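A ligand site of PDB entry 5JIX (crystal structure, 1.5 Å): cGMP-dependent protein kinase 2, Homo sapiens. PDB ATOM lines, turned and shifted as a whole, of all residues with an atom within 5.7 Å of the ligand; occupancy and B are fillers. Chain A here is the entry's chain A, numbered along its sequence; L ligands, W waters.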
ATOM      1  N   ILE A  48      11.658   6.704   8.050  1.00  0.00           N
ATOM      2  CA  ILE A  48      10.471   7.380   8.559  1.00  0.00           C
ATOM      3  C   ILE A  48      10.299   8.666   7.768  1.00  0.00           C
ATOM      4  O   ILE A  48      11.283   9.368   7.506  1.00  0.00           O
ATOM      5  CB  ILE A  48      10.635   7.692  10.058  1.00  0.00           C
ATOM      6  CG1 ILE A  48      10.557   6.393  10.870  1.00  0.00           C
ATOM      7  CG2 ILE A  48       9.616   8.690  10.489  1.00  0.00           C
ATOM      8  CD1 ILE A  48      10.605   6.587  12.383  1.00  0.00           C
ATOM      9  N   VAL A  67      18.503  12.840  10.599  1.00  0.00           N
ATOM     10  CA  VAL A  67      17.208  13.293  11.082  1.00  0.00           C
ATOM     11  C   VAL A  67      17.001  14.663  10.457  1.00  0.00           C
ATOM     12  O   VAL A  67      17.811  15.568  10.669  1.00  0.00           O
ATOM     13  CB  VAL A  67      17.178  13.427  12.612  1.00  0.00           C
ATOM     14  CG1 VAL A  67      15.773  13.809  13.081  1.00  0.00           C
ATOM     15  CG2 VAL A  67      17.650  12.150  13.302  1.00  0.00           C
ATOM     16  N   GLN A  69      13.835  17.754   9.514  1.00  0.00           N
ATOM     17  CA  GLN A  69      12.512  18.185   9.937  1.00  0.00           C
ATOM     18  C   GLN A  69      12.141  19.476   9.228  1.00  0.00           C
ATOM     19  O   GLN A  69      12.992  20.356   9.061  1.00  0.00           O
ATOM     20  CB  GLN A  69      12.524  18.417  11.445  1.00  0.00           C
ATOM     21  CG  GLN A  69      11.172  18.656  12.072  1.00  0.00           C
ATOM     22  CD  GLN A  69      11.305  18.821  13.572  1.00  0.00           C
ATOM     23  OE1 GLN A  69      12.017  19.706  14.041  1.00  0.00           O
ATOM     24  NE2 GLN A  69      10.685  17.939  14.329  1.00  0.00           N
ATOM     25  N   ILE A  80      18.847  18.055  11.446  1.00  0.00           N
ATOM     26  CA  ILE A  80      18.817  18.259  12.893  1.00  0.00           C
ATOM     27  C   ILE A  80      19.978  17.564  13.573  1.00  0.00           C
ATOM     28  O   ILE A  80      20.614  18.137  14.475  1.00  0.00           O
ATOM     29  CB  ILE A  80      17.471  17.738  13.438  1.00  0.00           C
ATOM     30  CG1 ILE A  80      16.296  18.352  12.686  1.00  0.00           C
ATOM     31  CG2 ILE A  80      17.414  17.955  14.933  1.00  0.00           C
ATOM     32  CD1 ILE A  80      16.318  19.821  12.567  1.00  0.00           C
ATOM     33  N   LYS A  81      20.257  16.320  13.211  1.00  0.00           N
ATOM     34  CA  LYS A  81      21.312  15.525  13.820  1.00  0.00           C
ATOM     35  C   LYS A  81      21.476  14.267  12.968  1.00  0.00           C
ATOM     36  O   LYS A  81      20.718  14.043  12.030  1.00  0.00           O
ATOM     37  CB  LYS A  81      20.958  15.138  15.260  1.00  0.00           C
ATOM     38  CG  LYS A  81      19.761  14.178  15.377  1.00  0.00           C
ATOM     39  CD  LYS A  81      19.274  14.043  16.812  1.00  0.00           C
ATOM     40  CE  LYS A  81      18.620  15.319  17.295  1.00  0.00           C
ATOM     41  NZ  LYS A  81      18.028  15.105  18.668  1.00  0.00           N
ATOM     42  N   LEU A  83      22.337   9.886  13.568  1.00  0.00           N
ATOM     43  CA  LEU A  83      22.370   8.811  14.535  1.00  0.00           C
ATOM     44  C   LEU A  83      23.227   7.687  13.994  1.00  0.00           C
ATOM     45  O   LEU A  83      23.406   7.549  12.782  1.00  0.00           O
ATOM     46  CB  LEU A  83      20.972   8.247  14.800  1.00  0.00           C
ATOM     47  CG  LEU A  83      19.877   9.256  15.107  1.00  0.00           C
ATOM     48  CD1 LEU A  83      18.572   8.520  15.226  1.00  0.00           C
ATOM     49  CD2 LEU A  83      20.178  10.095  16.362  1.00  0.00           C
ATOM     50  N   TYR A  88      18.288   4.804  18.751  1.00  0.00           N
ATOM     51  CA  TYR A  88      16.930   4.405  18.439  1.00  0.00           C
ATOM     52  C   TYR A  88      16.084   5.612  18.068  1.00  0.00           C
ATOM     53  O   TYR A  88      16.462   6.764  18.300  1.00  0.00           O
ATOM     54  CB  TYR A  88      16.318   3.662  19.626  1.00  0.00           C
ATOM     55  CG  TYR A  88      16.292   4.427  20.919  1.00  0.00           C
ATOM     56  CD1 TYR A  88      15.308   5.378  21.179  1.00  0.00           C
ATOM     57  CD2 TYR A  88      17.251   4.200  21.893  1.00  0.00           C
ATOM     58  CE1 TYR A  88      15.278   6.079  22.374  1.00  0.00           C
ATOM     59  CE2 TYR A  88      17.233   4.885  23.080  1.00  0.00           C
ATOM     60  CZ  TYR A  88      16.252   5.808  23.324  1.00  0.00           C
ATOM     61  OH  TYR A  88      16.248   6.498  24.512  1.00  0.00           O
ATOM     62  N   PHE A  89      14.925   5.353  17.492  1.00  0.00           N
ATOM     63  CA  PHE A  89      14.050   6.416  17.006  1.00  0.00           C
ATOM     64  C   PHE A  89      12.672   5.838  16.702  1.00  0.00           C
ATOM     65  O   PHE A  89      12.492   4.626  16.572  1.00  0.00           O
ATOM     66  CB  PHE A  89      14.613   7.153  15.779  1.00  0.00           C
ATOM     67  CG  PHE A  89      14.943   6.258  14.621  1.00  0.00           C
ATOM     68  CD1 PHE A  89      13.972   5.959  13.677  1.00  0.00           C
ATOM     69  CD2 PHE A  89      16.202   5.688  14.483  1.00  0.00           C
ATOM     70  CE1 PHE A  89      14.259   5.115  12.628  1.00  0.00           C
ATOM     71  CE2 PHE A  89      16.478   4.811  13.418  1.00  0.00           C
ATOM     72  CZ  PHE A  89      15.507   4.553  12.491  1.00  0.00           C
ATOM     73  N   GLY A  90      11.685   6.741  16.604  1.00  0.00           N
ATOM     74  CA  GLY A  90      10.300   6.370  16.384  1.00  0.00           C
ATOM     75  C   GLY A  90       9.455   6.202  17.619  1.00  0.00           C
ATOM     76  O   GLY A  90       8.256   5.934  17.498  1.00  0.00           O
ATOM     77  N   GLU A  91      10.035   6.379  18.812  1.00  0.00           N
ATOM     78  CA  GLU A  91       9.253   6.288  20.039  1.00  0.00           C
ATOM     79  C   GLU A  91       8.257   7.433  20.177  1.00  0.00           C
ATOM     80  O   GLU A  91       7.221   7.281  20.824  1.00  0.00           O
ATOM     81  CB  GLU A  91      10.166   6.257  21.267  1.00  0.00           C
ATOM     82  CG  GLU A  91      10.805   7.601  21.580  1.00  0.00           C
ATOM     83  CD  GLU A  91      11.728   8.093  20.463  1.00  0.00           C
ATOM     84  OE1 GLU A  91      12.632   7.314  20.080  1.00  0.00           O
ATOM     85  OE2 GLU A  91      11.510   9.228  19.960  1.00  0.00           O
ATOM     86  N   LYS A  92       8.528   8.574  19.546  1.00  0.00           N
ATOM     87  CA  LYS A  92       7.713   9.750  19.836  1.00  0.00           C
ATOM     88  C   LYS A  92       6.282   9.572  19.355  1.00  0.00           C
ATOM     89  O   LYS A  92       5.342  10.024  20.027  1.00  0.00           O
ATOM     90  CB  LYS A  92       8.345  11.009  19.265  1.00  0.00           C
ATOM     91  CG  LYS A  92       7.671  12.280  19.759  1.00  0.00           C
ATOM     92  CD  LYS A  92       8.324  13.526  19.151  1.00  0.00           C
ATOM     93  CE  LYS A  92       7.942  14.802  19.819  1.00  0.00           C
ATOM     94  NZ  LYS A  92       6.455  15.015  19.961  1.00  0.00           N
ATOM     95  N   ALA A  93       6.065   8.956  18.202  1.00  0.00           N
ATOM     96  CA  ALA A  93       4.701   8.781  17.714  1.00  0.00           C
ATOM     97  C   ALA A  93       3.895   7.983  18.740  1.00  0.00           C
ATOM     98  O   ALA A  93       2.714   8.276  18.973  1.00  0.00           O
ATOM     99  CB  ALA A  93       4.730   8.074  16.365  1.00  0.00           C
ATOM    100  N   LEU A  94       4.532   7.007  19.385  1.00  0.00           N
ATOM    101  CA  LEU A  94       3.841   6.203  20.401  1.00  0.00           C
ATOM    102  C   LEU A  94       3.563   7.006  21.666  1.00  0.00           C
ATOM    103  O   LEU A  94       2.465   6.952  22.223  1.00  0.00           O
ATOM    104  CB  LEU A  94       4.683   4.967  20.726  1.00  0.00           C
ATOM    105  CG  LEU A  94       4.942   4.040  19.530  1.00  0.00           C
ATOM    106  CD1 LEU A  94       5.958   2.949  19.879  1.00  0.00           C
ATOM    107  CD2 LEU A  94       3.645   3.416  19.042  1.00  0.00           C
ATOM    108  N   VAL A  99       1.294  11.456  14.510  1.00  0.00           N
ATOM    109  CA  VAL A  99       1.980  11.046  13.301  1.00  0.00           C
ATOM    110  C   VAL A  99       3.477  11.294  13.464  1.00  0.00           C
ATOM    111  O   VAL A  99       3.913  11.967  14.398  1.00  0.00           O
ATOM    112  CB  VAL A  99       1.436  11.779  12.061  1.00  0.00           C
ATOM    113  CG1 VAL A  99      -0.061  11.530  11.898  1.00  0.00           C
ATOM    114  CG2 VAL A  99       1.755  13.264  12.135  1.00  0.00           C
ATOM    115  N   ARG A 100       4.257  10.741  12.558  1.00  0.00           N
ATOM    116  CA  ARG A 100       5.709  10.914  12.605  1.00  0.00           C
ATOM    117  C   ARG A 100       6.071  12.396  12.497  1.00  0.00           C
ATOM    118  O   ARG A 100       5.506  13.134  11.690  1.00  0.00           O
ATOM    119  CB  ARG A 100       6.348  10.163  11.450  1.00  0.00           C
ATOM    120  CG  ARG A 100       6.122   8.663  11.453  1.00  0.00           C
ATOM    121  CD  ARG A 100       6.679   7.999  12.703  1.00  0.00           C
ATOM    122  NE  ARG A 100       6.788   6.544  12.511  1.00  0.00           N
ATOM    123  CZ  ARG A 100       7.138   5.701  13.471  1.00  0.00           C
ATOM    124  NH1 ARG A 100       7.419   6.130  14.669  1.00  0.00           N
ATOM    125  NH2 ARG A 100       7.196   4.396  13.216  1.00  0.00           N
ATOM    126  N   SER A 101       7.048  12.817  13.296  1.00  0.00           N
ATOM    127  CA  SER A 101       7.311  14.238  13.484  1.00  0.00           C
ATOM    128  C   SER A 101       8.616  14.692  12.860  1.00  0.00           C
ATOM    129  O   SER A 101       8.965  15.870  12.997  1.00  0.00           O
ATOM    130  CB  SER A 101       7.279  14.598  14.967  1.00  0.00           C
ATOM    131  OG  SER A 101       8.242  13.864  15.670  1.00  0.00           O
ATOM    132  N   ALA A 102       9.338  13.791  12.212  1.00  0.00           N
ATOM    133  CA  ALA A 102      10.594  14.108  11.544  1.00  0.00           C
ATOM    134  C   ALA A 102      10.860  12.998  10.542  1.00  0.00           C
ATOM    135  O   ALA A 102      10.236  11.927  10.574  1.00  0.00           O
ATOM    136  CB  ALA A 102      11.750  14.195  12.544  1.00  0.00           C
ATOM    137  N   ASN A 103      11.765  13.291   9.611  1.00  0.00           N
ATOM    138  CA  ASN A 103      12.211  12.259   8.687  1.00  0.00           C
ATOM    139  C   ASN A 103      13.461  11.594   9.241  1.00  0.00           C
ATOM    140  O   ASN A 103      14.325  12.251   9.828  1.00  0.00           O
ATOM    141  CB  ASN A 103      12.558  12.873   7.341  1.00  0.00           C
ATOM    142  CG  ASN A 103      11.453  13.743   6.785  1.00  0.00           C
ATOM    143  OD1 ASN A 103      10.370  13.266   6.447  1.00  0.00           O
ATOM    144  ND2 ASN A 103      11.725  15.055   6.664  1.00  0.00           N
ATOM    145  N   ILE A 104      13.584  10.296   9.003  1.00  0.00           N
ATOM    146  CA  ILE A 104      14.815   9.559   9.290  1.00  0.00           C
ATOM    147  C   ILE A 104      15.267   8.950   7.957  1.00  0.00           C
ATOM    148  O   ILE A 104      14.521   8.174   7.342  1.00  0.00           O
ATOM    149  CB  ILE A 104      14.613   8.444  10.339  1.00  0.00           C
ATOM    150  CG1 ILE A 104      13.960   8.968  11.623  1.00  0.00           C
ATOM    151  CG2 ILE A 104      15.935   7.828  10.671  1.00  0.00           C
ATOM    152  CD1 ILE A 104      14.825   9.922  12.454  1.00  0.00           C
ATOM    153  N   TYR A 138      12.379  12.370  27.685  1.00  0.00           N
ATOM    154  CA  TYR A 138      13.101  12.528  26.429  1.00  0.00           C
ATOM    155  C   TYR A 138      12.206  13.178  25.372  1.00  0.00           C
ATOM    156  O   TYR A 138      12.608  14.121  24.677  1.00  0.00           O
ATOM    157  CB  TYR A 138      13.584  11.157  25.977  1.00  0.00           C
ATOM    158  CG  TYR A 138      14.175  11.119  24.588  1.00  0.00           C
ATOM    159  CD1 TYR A 138      15.288  11.864  24.259  1.00  0.00           C
ATOM    160  CD2 TYR A 138      13.594  10.351  23.608  1.00  0.00           C
ATOM    161  CE1 TYR A 138      15.820  11.818  22.958  1.00  0.00           C
ATOM    162  CE2 TYR A 138      14.108  10.290  22.329  1.00  0.00           C
ATOM    163  CZ  TYR A 138      15.208  11.028  22.017  1.00  0.00           C
ATOM    164  OH  TYR A 138      15.700  10.965  20.732  1.00  0.00           O
ATOM    165  N   LEU A 142      12.461  16.613  23.189  1.00  0.00           N
ATOM    166  CA  LEU A 142      12.258  16.730  21.734  1.00  0.00           C
ATOM    167  C   LEU A 142      11.225  17.804  21.423  1.00  0.00           C
ATOM    168  O   LEU A 142      11.375  18.586  20.476  1.00  0.00           O
ATOM    169  CB  LEU A 142      11.840  15.376  21.150  1.00  0.00           C
ATOM    170  CG  LEU A 142      12.839  14.229  21.216  1.00  0.00           C
ATOM    171  CD1 LEU A 142      12.287  13.039  20.439  1.00  0.00           C
ATOM    172  CD2 LEU A 142      14.234  14.631  20.675  1.00  0.00           C
ATOM    173  N   ASP A 145      12.939  21.089  21.733  1.00  0.00           N
ATOM    174  CA  ASP A 145      13.820  21.338  20.591  1.00  0.00           C
ATOM    175  C   ASP A 145      13.001  21.720  19.374  1.00  0.00           C
ATOM    176  O   ASP A 145      13.407  22.597  18.587  1.00  0.00           O
ATOM    177  CB  ASP A 145      14.615  20.075  20.277  1.00  0.00           C
ATOM    178  CG  ASP A 145      15.625  19.713  21.357  1.00  0.00           C
ATOM    179  OD1 ASP A 145      15.970  20.544  22.219  1.00  0.00           O
ATOM    180  OD2 ASP A 145      16.105  18.558  21.313  1.00  0.00           O
ATOM    181  N   ASP A 146      11.872  21.046  19.154  1.00  0.00           N
ATOM    182  CA  ASP A 146      10.992  21.338  18.030  1.00  0.00           C
ATOM    183  C   ASP A 146      10.498  22.768  18.105  1.00  0.00           C
ATOM    184  O   ASP A 146      10.517  23.502  17.113  1.00  0.00           O
ATOM    185  CB  ASP A 146       9.786  20.396  17.998  1.00  0.00           C
ATOM    186  CG  ASP A 146      10.127  18.981  17.578  1.00  0.00           C
ATOM    187  OD1 ASP A 146      11.284  18.746  17.178  1.00  0.00           O
ATOM    188  OD2 ASP A 146       9.212  18.139  17.671  1.00  0.00           O
ATOM    189  N   ARG A 149      13.279  25.467  17.315  1.00  0.00           N
ATOM    190  CA  ARG A 149      13.625  25.619  15.898  1.00  0.00           C
ATOM    191  C   ARG A 149      12.411  25.944  15.038  1.00  0.00           C
ATOM    192  O   ARG A 149      12.541  25.971  13.806  1.00  0.00           O
ATOM    193  CB  ARG A 149      14.338  24.370  15.353  1.00  0.00           C
ATOM    194  CG  ARG A 149      13.434  23.175  15.158  1.00  0.00           C
ATOM    195  CD  ARG A 149      14.186  21.997  14.530  1.00  0.00           C
ATOM    196  NE  ARG A 149      15.172  21.456  15.473  1.00  0.00           N
ATOM    197  CZ  ARG A 149      15.022  20.386  16.253  1.00  0.00           C
ATOM    198  NH1 ARG A 149      13.910  19.645  16.261  1.00  0.00           N
ATOM    199  NH2 ARG A 149      16.005  20.061  17.071  1.00  0.00           N
HETATM  200 BR1  LIG L   1      16.390  11.331  16.902  1.00  0.00          BR
HETATM  201  C1  LIG L   1      15.064  12.754  16.823  1.00  0.00           C
HETATM  202  N1  LIG L   1      15.386  14.019  17.097  1.00  0.00           N
HETATM  203  C2  LIG L   1      14.197  14.619  17.045  1.00  0.00           C
HETATM  204  C3  LIG L   1      13.698  15.966  17.242  1.00  0.00           C
HETATM  205  O1  LIG L   1      14.480  16.924  17.522  1.00  0.00           O
HETATM  206  N2  LIG L   1      12.392  16.154  17.130  1.00  0.00           N
HETATM  207  C4  LIG L   1      11.512  15.202  16.837  1.00  0.00           C
HETATM  208  N3  LIG L   1      10.237  15.557  16.732  1.00  0.00           N
HETATM  209  N4  LIG L   1      11.865  13.928  16.631  1.00  0.00           N
HETATM  210  C5  LIG L   1      13.155  13.614  16.731  1.00  0.00           C
HETATM  211  N5  LIG L   1      13.793  12.462  16.612  1.00  0.00           N
HETATM  212  C6  LIG L   1      13.223  11.160  16.269  1.00  0.00           C
HETATM  213  C7  LIG L   1      12.108  10.740  17.203  1.00  0.00           C
HETATM  214  O2  LIG L   1      12.394   9.416  17.611  1.00  0.00           O
HETATM  215  O3  LIG L   1      12.673  11.255  14.924  1.00  0.00           O
HETATM  216  C8  LIG L   1      11.504  10.440  14.911  1.00  0.00           C
HETATM  217  C9  LIG L   1      10.449  10.692  13.850  1.00  0.00           C
HETATM  218  O4  LIG L   1       9.392   9.751  14.100  1.00  0.00           O
HETATM  219  C10 LIG L   1      10.922  10.735  16.269  1.00  0.00           C
HETATM  220  O5  LIG L   1       9.878   9.838  16.555  1.00  0.00           O
HETATM  221  P1  LIG L   1       8.665   9.895  15.538  1.00  0.00           P
HETATM  222  O6  LIG L   1       7.774   8.702  15.705  1.00  0.00           O
HETATM  223  O7  LIG L   1       7.965  11.232  15.570  1.00  0.00           O
HETATM  224  O   HOH W   1      14.947   8.822  19.481  1.00  0.00           O
HETATM  225  O   HOH W   2       5.536  11.883  16.627  1.00  0.00           O
HETATM  226  O   HOH W   3      16.677  17.497  18.908  1.00  0.00           O
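OE2 of Glu 91 lies within hydrogen-bond range of O2 of the ligand.
An oxygen (O7) of the ligand sits at hydrogen-bond distance from the backbone NH (N) of Ser 101.
OG of Ser 101 is in hydrogen-bond range of O7 of the ligand (2.6 Å).
NH1 of Arg 100 lies within salt-bridge range of O6 of the ligand.
The side-chain carboxylate (OD1) of Asp 146 sits at hydrogen-bond distance from a nitrogen (N2) of the ligand, at 2.8 Å.
An oxygen (O2) of the ligand is in hydrogen-bond range of the backbone NH (N) of Gly 90 (2.9 Å).
The backbone NH of Ala 93 is in hydrogen-bond range of an oxygen (O6) of the ligand (3.0 Å).
NH1 of Arg 149 is in hydrogen-bond range of O1 of the ligand, 3.1 Å away.
NZ of Lys 81 is in hydrogen-bond range of N1 of the ligand, 3.3 Å away.
N3 of the ligand lies close to NE2 of Gln 69 (3.4 Å).
The backbone carbonyl oxygen (O) of Ser 101 lies within hydrogen-bond range of the side-chain amide nitrogen (NE2) of Gln 69 (3.0 Å).
The guanidinium group (NH1) of Arg 100 is in hydrogen-bond range of the backbone carbonyl oxygen (O) of Gly 90 (3.0 Å).
NH1 of Arg 149 lies within salt-bridge range of OD1 of Asp 146 (2.9 Å).
The side-chain carboxylate of Asp 146 lies within hydrogen-bond range of the side-chain amide nitrogen of Gln 69, 3.0 Å away.
The side-chain amide oxygen (OE1) of Gln 69 sits at hydrogen-bond distance from the guanidinium group (NH1) of Arg 149, 2.9 Å away.
O of Lys 81 sits at hydrogen-bond distance from N of Val 67 (2.9 Å).
The backbone NH (N) of Ile 104 lies within hydrogen-bond range of the backbone carbonyl oxygen (O) of Ile 48 (2.9 Å).
The backbone NH (N) of Ile 80 sits at hydrogen-bond distance from the backbone carbonyl oxygen (O) of Val 67 (2.8 Å).
Residues that only touch the ligand: Lys 92 (3.3 Å), Phe 89 (3.5 Å), Ala 102 (3.5 Å), Ile 104 (3.5 Å), Leu 142 (3.6 Å), Ile 48 (3.8 Å), Val 67 (3.9 Å), Tyr 138 (3.9 Å) and Leu 83 (3.9 Å).
Water W3 lies within hydrogen-bond range of an oxygen (O1) of the ligand (2.7 Å), the side-chain carboxylate of Asp 145 (2.7 Å), the side-chain amino group of Lys 81 (2.8 Å) and the guanidinium group of Arg 149 (3.2 Å).
Water W2 lies within hydrogen-bond range of O7 of the ligand, O of Val 99, N of Ala 93 and OG of Ser 101.
Water W1 lies within hydrogen-bond range of the side-chain hydroxyl (OH) of Tyr 138, the backbone carbonyl oxygen (O) of Tyr 88, the side-chain carboxylate (OE1) of Glu 91 and an oxygen (O2) of the ligand.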
